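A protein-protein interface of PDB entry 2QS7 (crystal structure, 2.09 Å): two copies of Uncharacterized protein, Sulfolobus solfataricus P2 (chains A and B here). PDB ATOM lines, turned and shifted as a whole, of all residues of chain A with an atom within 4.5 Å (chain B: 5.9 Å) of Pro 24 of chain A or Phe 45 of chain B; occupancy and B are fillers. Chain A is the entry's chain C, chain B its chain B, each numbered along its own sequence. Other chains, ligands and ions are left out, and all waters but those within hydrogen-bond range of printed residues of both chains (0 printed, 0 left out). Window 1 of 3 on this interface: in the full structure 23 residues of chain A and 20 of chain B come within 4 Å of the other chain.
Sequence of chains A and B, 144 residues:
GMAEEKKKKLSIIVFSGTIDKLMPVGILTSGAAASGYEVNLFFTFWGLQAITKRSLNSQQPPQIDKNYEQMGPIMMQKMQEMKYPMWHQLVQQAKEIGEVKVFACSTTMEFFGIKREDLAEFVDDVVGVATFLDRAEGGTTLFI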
ATOM      1  N   ASP A  20     -20.216  -4.961  -9.719  1.00  0.00           N
ATOM      2  CA  ASP A  20     -20.001  -4.033 -10.822  1.00  0.00           C
ATOM      3  C   ASP A  20     -21.320  -3.482 -11.347  1.00  0.00           C
ATOM      4  O   ASP A  20     -21.325  -2.422 -11.959  1.00  0.00           O
ATOM      5  CB  ASP A  20     -19.170  -4.662 -11.953  1.00  0.00           C
ATOM      6  CG  ASP A  20     -19.804  -5.920 -12.518  1.00  0.00           C
ATOM      7  OD1 ASP A  20     -19.950  -6.895 -11.745  1.00  0.00           O
ATOM      8  OD2 ASP A  20     -20.147  -5.940 -13.733  1.00  0.00           O
ATOM      9  N   LYS A  21     -22.429  -4.184 -11.122  1.00  0.00           N
ATOM     10  CA  LYS A  21     -23.733  -3.648 -11.532  1.00  0.00           C
ATOM     11  C   LYS A  21     -24.442  -2.919 -10.403  1.00  0.00           C
ATOM     12  O   LYS A  21     -25.180  -1.980 -10.652  1.00  0.00           O
ATOM     13  CB  LYS A  21     -24.617  -4.725 -12.151  1.00  0.00           C
ATOM     14  CG  LYS A  21     -24.130  -5.112 -13.525  1.00  0.00           C
ATOM     15  CD  LYS A  21     -25.201  -5.755 -14.372  1.00  0.00           C
ATOM     16  CE  LYS A  21     -24.616  -6.207 -15.703  1.00  0.00           C
ATOM     17  NZ  LYS A  21     -25.629  -6.836 -16.601  1.00  0.00           N
ATOM     18  N   LEU A  22     -24.195  -3.316  -9.165  1.00  0.00           N
ATOM     19  CA  LEU A  22     -24.808  -2.644  -8.045  1.00  0.00           C
ATOM     20  C   LEU A  22     -24.203  -1.262  -7.841  1.00  0.00           C
ATOM     21  O   LEU A  22     -24.911  -0.374  -7.401  1.00  0.00           O
ATOM     22  CB  LEU A  22     -24.727  -3.504  -6.792  1.00  0.00           C
ATOM     23  CG  LEU A  22     -25.496  -4.829  -6.881  1.00  0.00           C
ATOM     24  CD1 LEU A  22     -25.078  -5.755  -5.723  1.00  0.00           C
ATOM     25  CD2 LEU A  22     -26.988  -4.598  -6.894  1.00  0.00           C
ATOM     26  N   MET A  23     -22.920  -1.066  -8.156  1.00  0.00           N
ATOM     27  CA  MET A  23     -22.288   0.264  -8.019  1.00  0.00           C
ATOM     28  C   MET A  23     -23.027   1.329  -8.878  1.00  0.00           C
ATOM     29  O   MET A  23     -23.379   2.392  -8.390  1.00  0.00           O
ATOM     30  CB  MET A  23     -20.787   0.233  -8.356  1.00  0.00           C
ATOM     31  CG  MET A  23     -19.827  -0.270  -7.249  1.00  0.00           C
ATOM     32  SD  MET A  23     -20.070   0.694  -5.557  1.00  0.00           S
ATOM     33  CE  MET A  23     -20.360   2.553  -6.182  1.00  0.00           C
ATOM     34  N   PRO A  24     -23.215   1.070 -10.177  1.00  0.00           N
ATOM     35  CA  PRO A  24     -24.011   1.998 -10.992  1.00  0.00           C
ATOM     36  C   PRO A  24     -25.375   2.334 -10.368  1.00  0.00           C
ATOM     37  O   PRO A  24     -25.825   3.488 -10.407  1.00  0.00           O
ATOM     38  CB  PRO A  24     -24.208   1.238 -12.306  1.00  0.00           C
ATOM     39  CG  PRO A  24     -23.132   0.275 -12.370  1.00  0.00           C
ATOM     40  CD  PRO A  24     -22.637  -0.008 -10.985  1.00  0.00           C
ATOM     41  N   VAL A  25     -26.047   1.339  -9.811  1.00  0.00           N
ATOM     42  CA  VAL A  25     -27.331   1.591  -9.172  1.00  0.00           C
ATOM     43  C   VAL A  25     -27.161   2.628  -8.057  1.00  0.00           C
ATOM     44  O   VAL A  25     -27.953   3.559  -7.930  1.00  0.00           O
ATOM     45  CB  VAL A  25     -27.951   0.311  -8.580  1.00  0.00           C
ATOM     46  CG1 VAL A  25     -29.162   0.652  -7.727  1.00  0.00           C
ATOM     47  CG2 VAL A  25     -28.316  -0.656  -9.690  1.00  0.00           C
ATOM     48  N   GLY A  26     -26.146   2.458  -7.225  1.00  0.00           N
ATOM     49  CA  GLY A  26     -25.895   3.418  -6.166  1.00  0.00           C
ATOM     50  C   GLY A  26     -25.529   4.798  -6.686  1.00  0.00           C
ATOM     51  O   GLY A  26     -26.008   5.820  -6.173  1.00  0.00           O
ATOM     52  N   ILE A  27     -24.686   4.827  -7.717  1.00  0.00           N
ATOM     53  CA  ILE A  27     -24.230   6.083  -8.303  1.00  0.00           C
ATOM     54  C   ILE A  27     -25.374   6.818  -8.985  1.00  0.00           C
ATOM     55  O   ILE A  27     -25.501   8.021  -8.850  1.00  0.00           O
ATOM     56  CB  ILE A  27     -23.055   5.851  -9.293  1.00  0.00           C
ATOM     57  CG1 ILE A  27     -21.845   5.251  -8.554  1.00  0.00           C
ATOM     58  CG2 ILE A  27     -22.654   7.168  -9.968  1.00  0.00           C
ATOM     59  CD1 ILE A  27     -20.700   4.839  -9.463  1.00  0.00           C
ATOM     60  N   LEU A  28     -26.186   6.097  -9.742  1.00  0.00           N
ATOM     61  CA  LEU A  28     -27.327   6.707 -10.401  1.00  0.00           C
ATOM     62  C   LEU A  28     -28.304   7.234  -9.371  1.00  0.00           C
ATOM     63  O   LEU A  28     -28.811   8.336  -9.507  1.00  0.00           O
ATOM     64  CB  LEU A  28     -28.064   5.701 -11.313  1.00  0.00           C
ATOM     65  CG  LEU A  28     -27.458   5.369 -12.685  1.00  0.00           C
ATOM     66  CD1 LEU A  28     -28.033   4.092 -13.302  1.00  0.00           C
ATOM     67  CD2 LEU A  28     -27.680   6.565 -13.591  1.00  0.00           C
ATOM     68  N   MET A  75     -10.437  -2.224  -9.816  1.00  0.00           N
ATOM     69  CA  MET A  75     -11.607  -1.480  -9.384  1.00  0.00           C
ATOM     70  C   MET A  75     -11.749  -1.457  -7.870  1.00  0.00           C
ATOM     71  O   MET A  75     -11.896  -0.384  -7.287  1.00  0.00           O
ATOM     72  CB  MET A  75     -12.874  -2.085 -10.001  1.00  0.00           C
ATOM     73  CG  MET A  75     -14.160  -1.434  -9.536  1.00  0.00           C
ATOM     74  SD  MET A  75     -15.662  -2.409 -10.231  1.00  0.00           S
ATOM     75  CE  MET A  75     -17.145  -1.618  -9.020  1.00  0.00           C
ATOM     76  N   VAL B  14     -23.894   2.905 -21.911  1.00  0.00           N
ATOM     77  CA  VAL B  14     -23.126   1.789 -22.423  1.00  0.00           C
ATOM     78  C   VAL B  14     -22.226   1.341 -21.283  1.00  0.00           C
ATOM     79  O   VAL B  14     -21.115   1.844 -21.079  1.00  0.00           O
ATOM     80  CB  VAL B  14     -22.284   2.184 -23.622  1.00  0.00           C
ATOM     81  CG1 VAL B  14     -21.585   0.963 -24.171  1.00  0.00           C
ATOM     82  CG2 VAL B  14     -23.135   2.871 -24.723  1.00  0.00           C
ATOM     83  N   PHE B  15     -22.749   0.428 -20.495  1.00  0.00           N
ATOM     84  CA  PHE B  15     -22.037  -0.108 -19.350  1.00  0.00           C
ATOM     85  C   PHE B  15     -21.146  -1.309 -19.681  1.00  0.00           C
ATOM     86  O   PHE B  15     -20.054  -1.487 -19.145  1.00  0.00           O
ATOM     87  CB  PHE B  15     -23.083  -0.531 -18.336  1.00  0.00           C
ATOM     88  CG  PHE B  15     -22.526  -1.376 -17.221  1.00  0.00           C
ATOM     89  CD1 PHE B  15     -22.064  -0.792 -16.080  1.00  0.00           C
ATOM     90  CD2 PHE B  15     -22.497  -2.753 -17.329  1.00  0.00           C
ATOM     91  CE1 PHE B  15     -21.560  -1.545 -15.068  1.00  0.00           C
ATOM     92  CE2 PHE B  15     -21.995  -3.524 -16.309  1.00  0.00           C
ATOM     93  CZ  PHE B  15     -21.528  -2.920 -15.184  1.00  0.00           C
ATOM     94  N   PHE B  43     -20.756   6.332 -21.946  1.00  0.00           N
ATOM     95  CA  PHE B  43     -19.887   5.208 -21.706  1.00  0.00           C
ATOM     96  C   PHE B  43     -19.400   5.207 -20.268  1.00  0.00           C
ATOM     97  O   PHE B  43     -18.784   6.171 -19.813  1.00  0.00           O
ATOM     98  CB  PHE B  43     -18.714   5.269 -22.689  1.00  0.00           C
ATOM     99  CG  PHE B  43     -19.082   4.917 -24.095  1.00  0.00           C
ATOM    100  CD1 PHE B  43     -19.594   5.867 -24.957  1.00  0.00           C
ATOM    101  CD2 PHE B  43     -18.920   3.622 -24.555  1.00  0.00           C
ATOM    102  CE1 PHE B  43     -19.950   5.514 -26.271  1.00  0.00           C
ATOM    103  CE2 PHE B  43     -19.266   3.253 -25.846  1.00  0.00           C
ATOM    104  CZ  PHE B  43     -19.778   4.198 -26.718  1.00  0.00           C
ATOM    105  N   THR B  44     -19.688   4.114 -19.567  1.00  0.00           N
ATOM    106  CA  THR B  44     -19.365   3.981 -18.164  1.00  0.00           C
ATOM    107  C   THR B  44     -18.834   2.590 -17.880  1.00  0.00           C
ATOM    108  O   THR B  44     -19.050   1.666 -18.661  1.00  0.00           O
ATOM    109  CB  THR B  44     -20.638   4.256 -17.341  1.00  0.00           C
ATOM    110  OG1 THR B  44     -20.308   4.259 -15.950  1.00  0.00           O
ATOM    111  CG2 THR B  44     -21.719   3.230 -17.625  1.00  0.00           C
ATOM    112  N   PHE B  45     -18.146   2.432 -16.759  1.00  0.00           N
ATOM    113  CA  PHE B  45     -17.539   1.147 -16.390  1.00  0.00           C
ATOM    114  C   PHE B  45     -16.840   0.412 -17.545  1.00  0.00           C
ATOM    115  O   PHE B  45     -15.918   0.938 -18.131  1.00  0.00           O
ATOM    116  CB  PHE B  45     -18.548   0.258 -15.664  1.00  0.00           C
ATOM    117  CG  PHE B  45     -18.725   0.632 -14.245  1.00  0.00           C
ATOM    118  CD1 PHE B  45     -19.591   1.662 -13.896  1.00  0.00           C
ATOM    119  CD2 PHE B  45     -18.007  -0.023 -13.256  1.00  0.00           C
ATOM    120  CE1 PHE B  45     -19.751   2.026 -12.580  1.00  0.00           C
ATOM    121  CE2 PHE B  45     -18.159   0.324 -11.944  1.00  0.00           C
ATOM    122  CZ  PHE B  45     -19.031   1.359 -11.596  1.00  0.00           C
ATOM    123  N   TRP B  46     -17.320  -0.766 -17.916  1.00  0.00           N
ATOM    124  CA  TRP B  46     -16.649  -1.556 -18.927  1.00  0.00           C
ATOM    125  C   TRP B  46     -16.758  -0.926 -20.298  1.00  0.00           C
ATOM    126  O   TRP B  46     -15.885  -1.107 -21.146  1.00  0.00           O
ATOM    127  CB  TRP B  46     -17.179  -2.985 -18.945  1.00  0.00           C
ATOM    128  CG  TRP B  46     -17.325  -3.551 -17.599  1.00  0.00           C
ATOM    129  CD1 TRP B  46     -18.476  -3.958 -17.008  1.00  0.00           C
ATOM    130  CD2 TRP B  46     -16.292  -3.727 -16.629  1.00  0.00           C
ATOM    131  NE1 TRP B  46     -18.227  -4.398 -15.734  1.00  0.00           N
ATOM    132  CE2 TRP B  46     -16.892  -4.269 -15.477  1.00  0.00           C
ATOM    133  CE3 TRP B  46     -14.921  -3.485 -16.626  1.00  0.00           C
ATOM    134  CZ2 TRP B  46     -16.169  -4.589 -14.339  1.00  0.00           C
ATOM    135  CZ3 TRP B  46     -14.205  -3.803 -15.503  1.00  0.00           C
ATOM    136  CH2 TRP B  46     -14.829  -4.346 -14.368  1.00  0.00           C
ATOM    137  N   GLY B  47     -17.839  -0.183 -20.530  1.00  0.00           N
ATOM    138  CA  GLY B  47     -18.019   0.491 -21.794  1.00  0.00           C
ATOM    139  C   GLY B  47     -16.995   1.598 -21.957  1.00  0.00           C
ATOM    140  O   GLY B  47     -16.500   1.827 -23.056  1.00  0.00           O
ATOM    141  N   LEU B  48     -16.688   2.300 -20.878  1.00  0.00           N
ATOM    142  CA  LEU B  48     -15.707   3.365 -20.943  1.00  0.00           C
ATOM    143  C   LEU B  48     -14.335   2.758 -21.292  1.00  0.00           C
ATOM    144  O   LEU B  48     -13.581   3.308 -22.096  1.00  0.00           O
ATOM    145  CB  LEU B  48     -15.662   4.113 -19.625  1.00  0.00           C
ATOM    146  CG  LEU B  48     -14.706   5.290 -19.538  1.00  0.00           C
ATOM    147  CD1 LEU B  48     -15.139   6.385 -20.482  1.00  0.00           C
ATOM    148  CD2 LEU B  48     -14.660   5.780 -18.132  1.00  0.00           C
ATOM    149  N   GLN B  49     -14.034   1.601 -20.716  1.00  0.00           N
ATOM    150  CA  GLN B  49     -12.774   0.911 -20.980  1.00  0.00           C
ATOM    151  C   GLN B  49     -12.686   0.628 -22.488  1.00  0.00           C
ATOM    152  O   GLN B  49     -11.630   0.746 -23.090  1.00  0.00           O
ATOM    153  CB  GLN B  49     -12.734  -0.394 -20.158  1.00  0.00           C
ATOM    154  CG  GLN B  49     -11.369  -0.987 -19.901  1.00  0.00           C
ATOM    155  CD  GLN B  49     -10.550  -0.194 -18.877  1.00  0.00           C
ATOM    156  OE1 GLN B  49     -11.103   0.415 -17.947  1.00  0.00           O
ATOM    157  NE2 GLN B  49      -9.226  -0.209 -19.042  1.00  0.00           N
ATOM    158  N   ALA B  50     -13.813   0.271 -23.085  1.00  0.00           N
ATOM    159  CA  ALA B  50     -13.889  -0.051 -24.507  1.00  0.00           C
ATOM    160  C   ALA B  50     -13.601   1.127 -25.460  1.00  0.00           C
ATOM    161  O   ALA B  50     -13.231   0.905 -26.615  1.00  0.00           O
ATOM    162  CB  ALA B  50     -15.254  -0.661 -24.815  1.00  0.00           C
ATOM    163  N   CYS B 105     -18.198   8.787 -18.762  1.00  0.00           N
ATOM    164  CA  CYS B 105     -18.543   8.926 -17.350  1.00  0.00           C
ATOM    165  C   CYS B 105     -17.333   9.308 -16.495  1.00  0.00           C
ATOM    166  O   CYS B 105     -16.363   8.571 -16.439  1.00  0.00           O
ATOM    167  CB  CYS B 105     -19.141   7.618 -16.843  1.00  0.00           C
ATOM    168  SG  CYS B 105     -19.309   7.540 -15.041  1.00  0.00           S
ATOM    169  N   THR B 108     -16.349   6.665 -13.352  1.00  0.00           N
ATOM    170  CA  THR B 108     -15.645   5.478 -13.789  1.00  0.00           C
ATOM    171  C   THR B 108     -14.213   5.829 -14.132  1.00  0.00           C
ATOM    172  O   THR B 108     -13.308   5.037 -13.878  1.00  0.00           O
ATOM    173  CB  THR B 108     -16.227   4.880 -15.089  1.00  0.00           C
ATOM    174  OG1 THR B 108     -17.645   4.742 -15.004  1.00  0.00           O
ATOM    175  CG2 THR B 108     -15.589   3.537 -15.374  1.00  0.00           C
ATOM    176  N   PHE B 111     -12.252   5.696 -11.002  1.00  0.00           N
ATOM    177  CA  PHE B 111     -12.099   4.297 -10.579  1.00  0.00           C
ATOM    178  C   PHE B 111     -11.032   3.537 -11.365  1.00  0.00           C
ATOM    179  O   PHE B 111     -10.305   2.736 -10.779  1.00  0.00           O
ATOM    180  CB  PHE B 111     -13.412   3.510 -10.754  1.00  0.00           C
ATOM    181  CG  PHE B 111     -14.481   3.800  -9.722  1.00  0.00           C
ATOM    182  CD1 PHE B 111     -14.361   4.846  -8.797  1.00  0.00           C
ATOM    183  CD2 PHE B 111     -15.693   3.081  -9.781  1.00  0.00           C
ATOM    184  CE1 PHE B 111     -15.388   5.108  -7.890  1.00  0.00           C
ATOM    185  CE2 PHE B 111     -16.741   3.346  -8.889  1.00  0.00           C
ATOM    186  CZ  PHE B 111     -16.589   4.363  -7.940  1.00  0.00           C
ATOM    187  N   PHE B 112     -10.956   3.743 -12.681  1.00  0.00           N
ATOM    188  CA  PHE B 112      -9.979   2.993 -13.494  1.00  0.00           C
ATOM    189  C   PHE B 112      -8.695   3.794 -13.828  1.00  0.00           C
ATOM    190  O   PHE B 112      -7.832   3.305 -14.575  1.00  0.00           O
ATOM    191  CB  PHE B 112     -10.619   2.424 -14.776  1.00  0.00           C
ATOM    192  CG  PHE B 112     -11.707   1.378 -14.531  1.00  0.00           C
ATOM    193  CD1 PHE B 112     -11.439   0.207 -13.834  1.00  0.00           C
ATOM    194  CD2 PHE B 112     -12.980   1.538 -15.059  1.00  0.00           C
ATOM    195  CE1 PHE B 112     -12.451  -0.753 -13.631  1.00  0.00           C
ATOM    196  CE2 PHE B 112     -13.984   0.573 -14.865  1.00  0.00           C
ATOM    197  CZ  PHE B 112     -13.727  -0.552 -14.156  1.00  0.00           C
ATOM    198  N   PHE B 143     -30.165   0.874 -20.814  1.00  0.00           N
ATOM    199  CA  PHE B 143     -28.949   0.529 -20.101  1.00  0.00           C
ATOM    200  C   PHE B 143     -28.496  -0.798 -20.717  1.00  0.00           C
ATOM    201  O   PHE B 143     -29.161  -1.833 -20.552  1.00  0.00           O
ATOM    202  CB  PHE B 143     -29.236   0.339 -18.619  1.00  0.00           C
ATOM    203  CG  PHE B 143     -28.012   0.065 -17.782  1.00  0.00           C
ATOM    204  CD1 PHE B 143     -27.521  -1.234 -17.644  1.00  0.00           C
ATOM    205  CD2 PHE B 143     -27.362   1.099 -17.117  1.00  0.00           C
ATOM    206  CE1 PHE B 143     -26.382  -1.503 -16.840  1.00  0.00           C
ATOM    207  CE2 PHE B 143     -26.229   0.831 -16.294  1.00  0.00           C
ATOM    208  CZ  PHE B 143     -25.751  -0.468 -16.165  1.00  0.00           C
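Of the printed residues of chain B, Asp 20 of chain A touches Phe 15 and Trp 46.
Of chain B, only Phe 15 (3.6 Å) and Phe 45 (3.8 Å) come within 4 Å of Pro 24 of chain A.
Of the printed residues of chain A, Phe 15 of chain B touches Asp 20, Lys 21 and Pro 24.
Phe 45 of chain B touches just these residues of chain A: Met 23 (3.9 Å), Pro 24 (3.8 Å) and Met 75 (3.7 Å).
Printed residues of chain A within 4 Å of Trp 46 of chain B: Asp 20.
Ala 50 of chain B touches none of the printed residues of chain A.
The nearest residue of chain A that does not touch Phe 45 of chain B is Asp 20 of chain A (4.2 Å).
The side-chain carboxylate (OD2) of Asp 20 of chain A sits at hydrogen-bond distance from the indole nitrogen (NE1) of Trp 46 of chain B (3.2 Å).
Of the 10 printed residues of chain A, 5 touch a printed residue of chain B.
Printed residues of chain B that touch a printed residue of chain A: Phe 15, Phe 45, Trp 46 and Phe 112.
Hydrophobic or aromatic side chains of chain B within 4 Å of the printed part of chain A: Phe 15, Phe 45, Trp 46 and Phe 112.
No position is printed for both chains.
Of the 8 pairs that touch across the chains among the printed residues, none has its exchanged pair printed and touching as well.
Among the printed residues, merely in contact across the chains: Asp 20 of chain A with Phe 15 of chain B, Lys 21 of chain A with Phe 15 of chain B, Met 23 of chain A with Phe 45 of chain B, Pro 24 of chain A with Phe 15 of chain B, Pro 24 of chain A with Phe 45 of chain B, Met 75 of chain A with Phe 45 of chain B and Met 75 of chain A with Phe 112 of chain B.
The backbone NH (N) of Gly 47 of chain B sits at hydrogen-bond distance from the backbone carbonyl oxygen (O) of Phe 15 of chain B.
O of Phe 15 of chain B lies within hydrogen-bond range of N of Trp 46 of chain B, at 3.1 Å.
N of Phe 45 of chain B sits at hydrogen-bond distance from OG1 of Thr 108 of chain B (2.9 Å).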
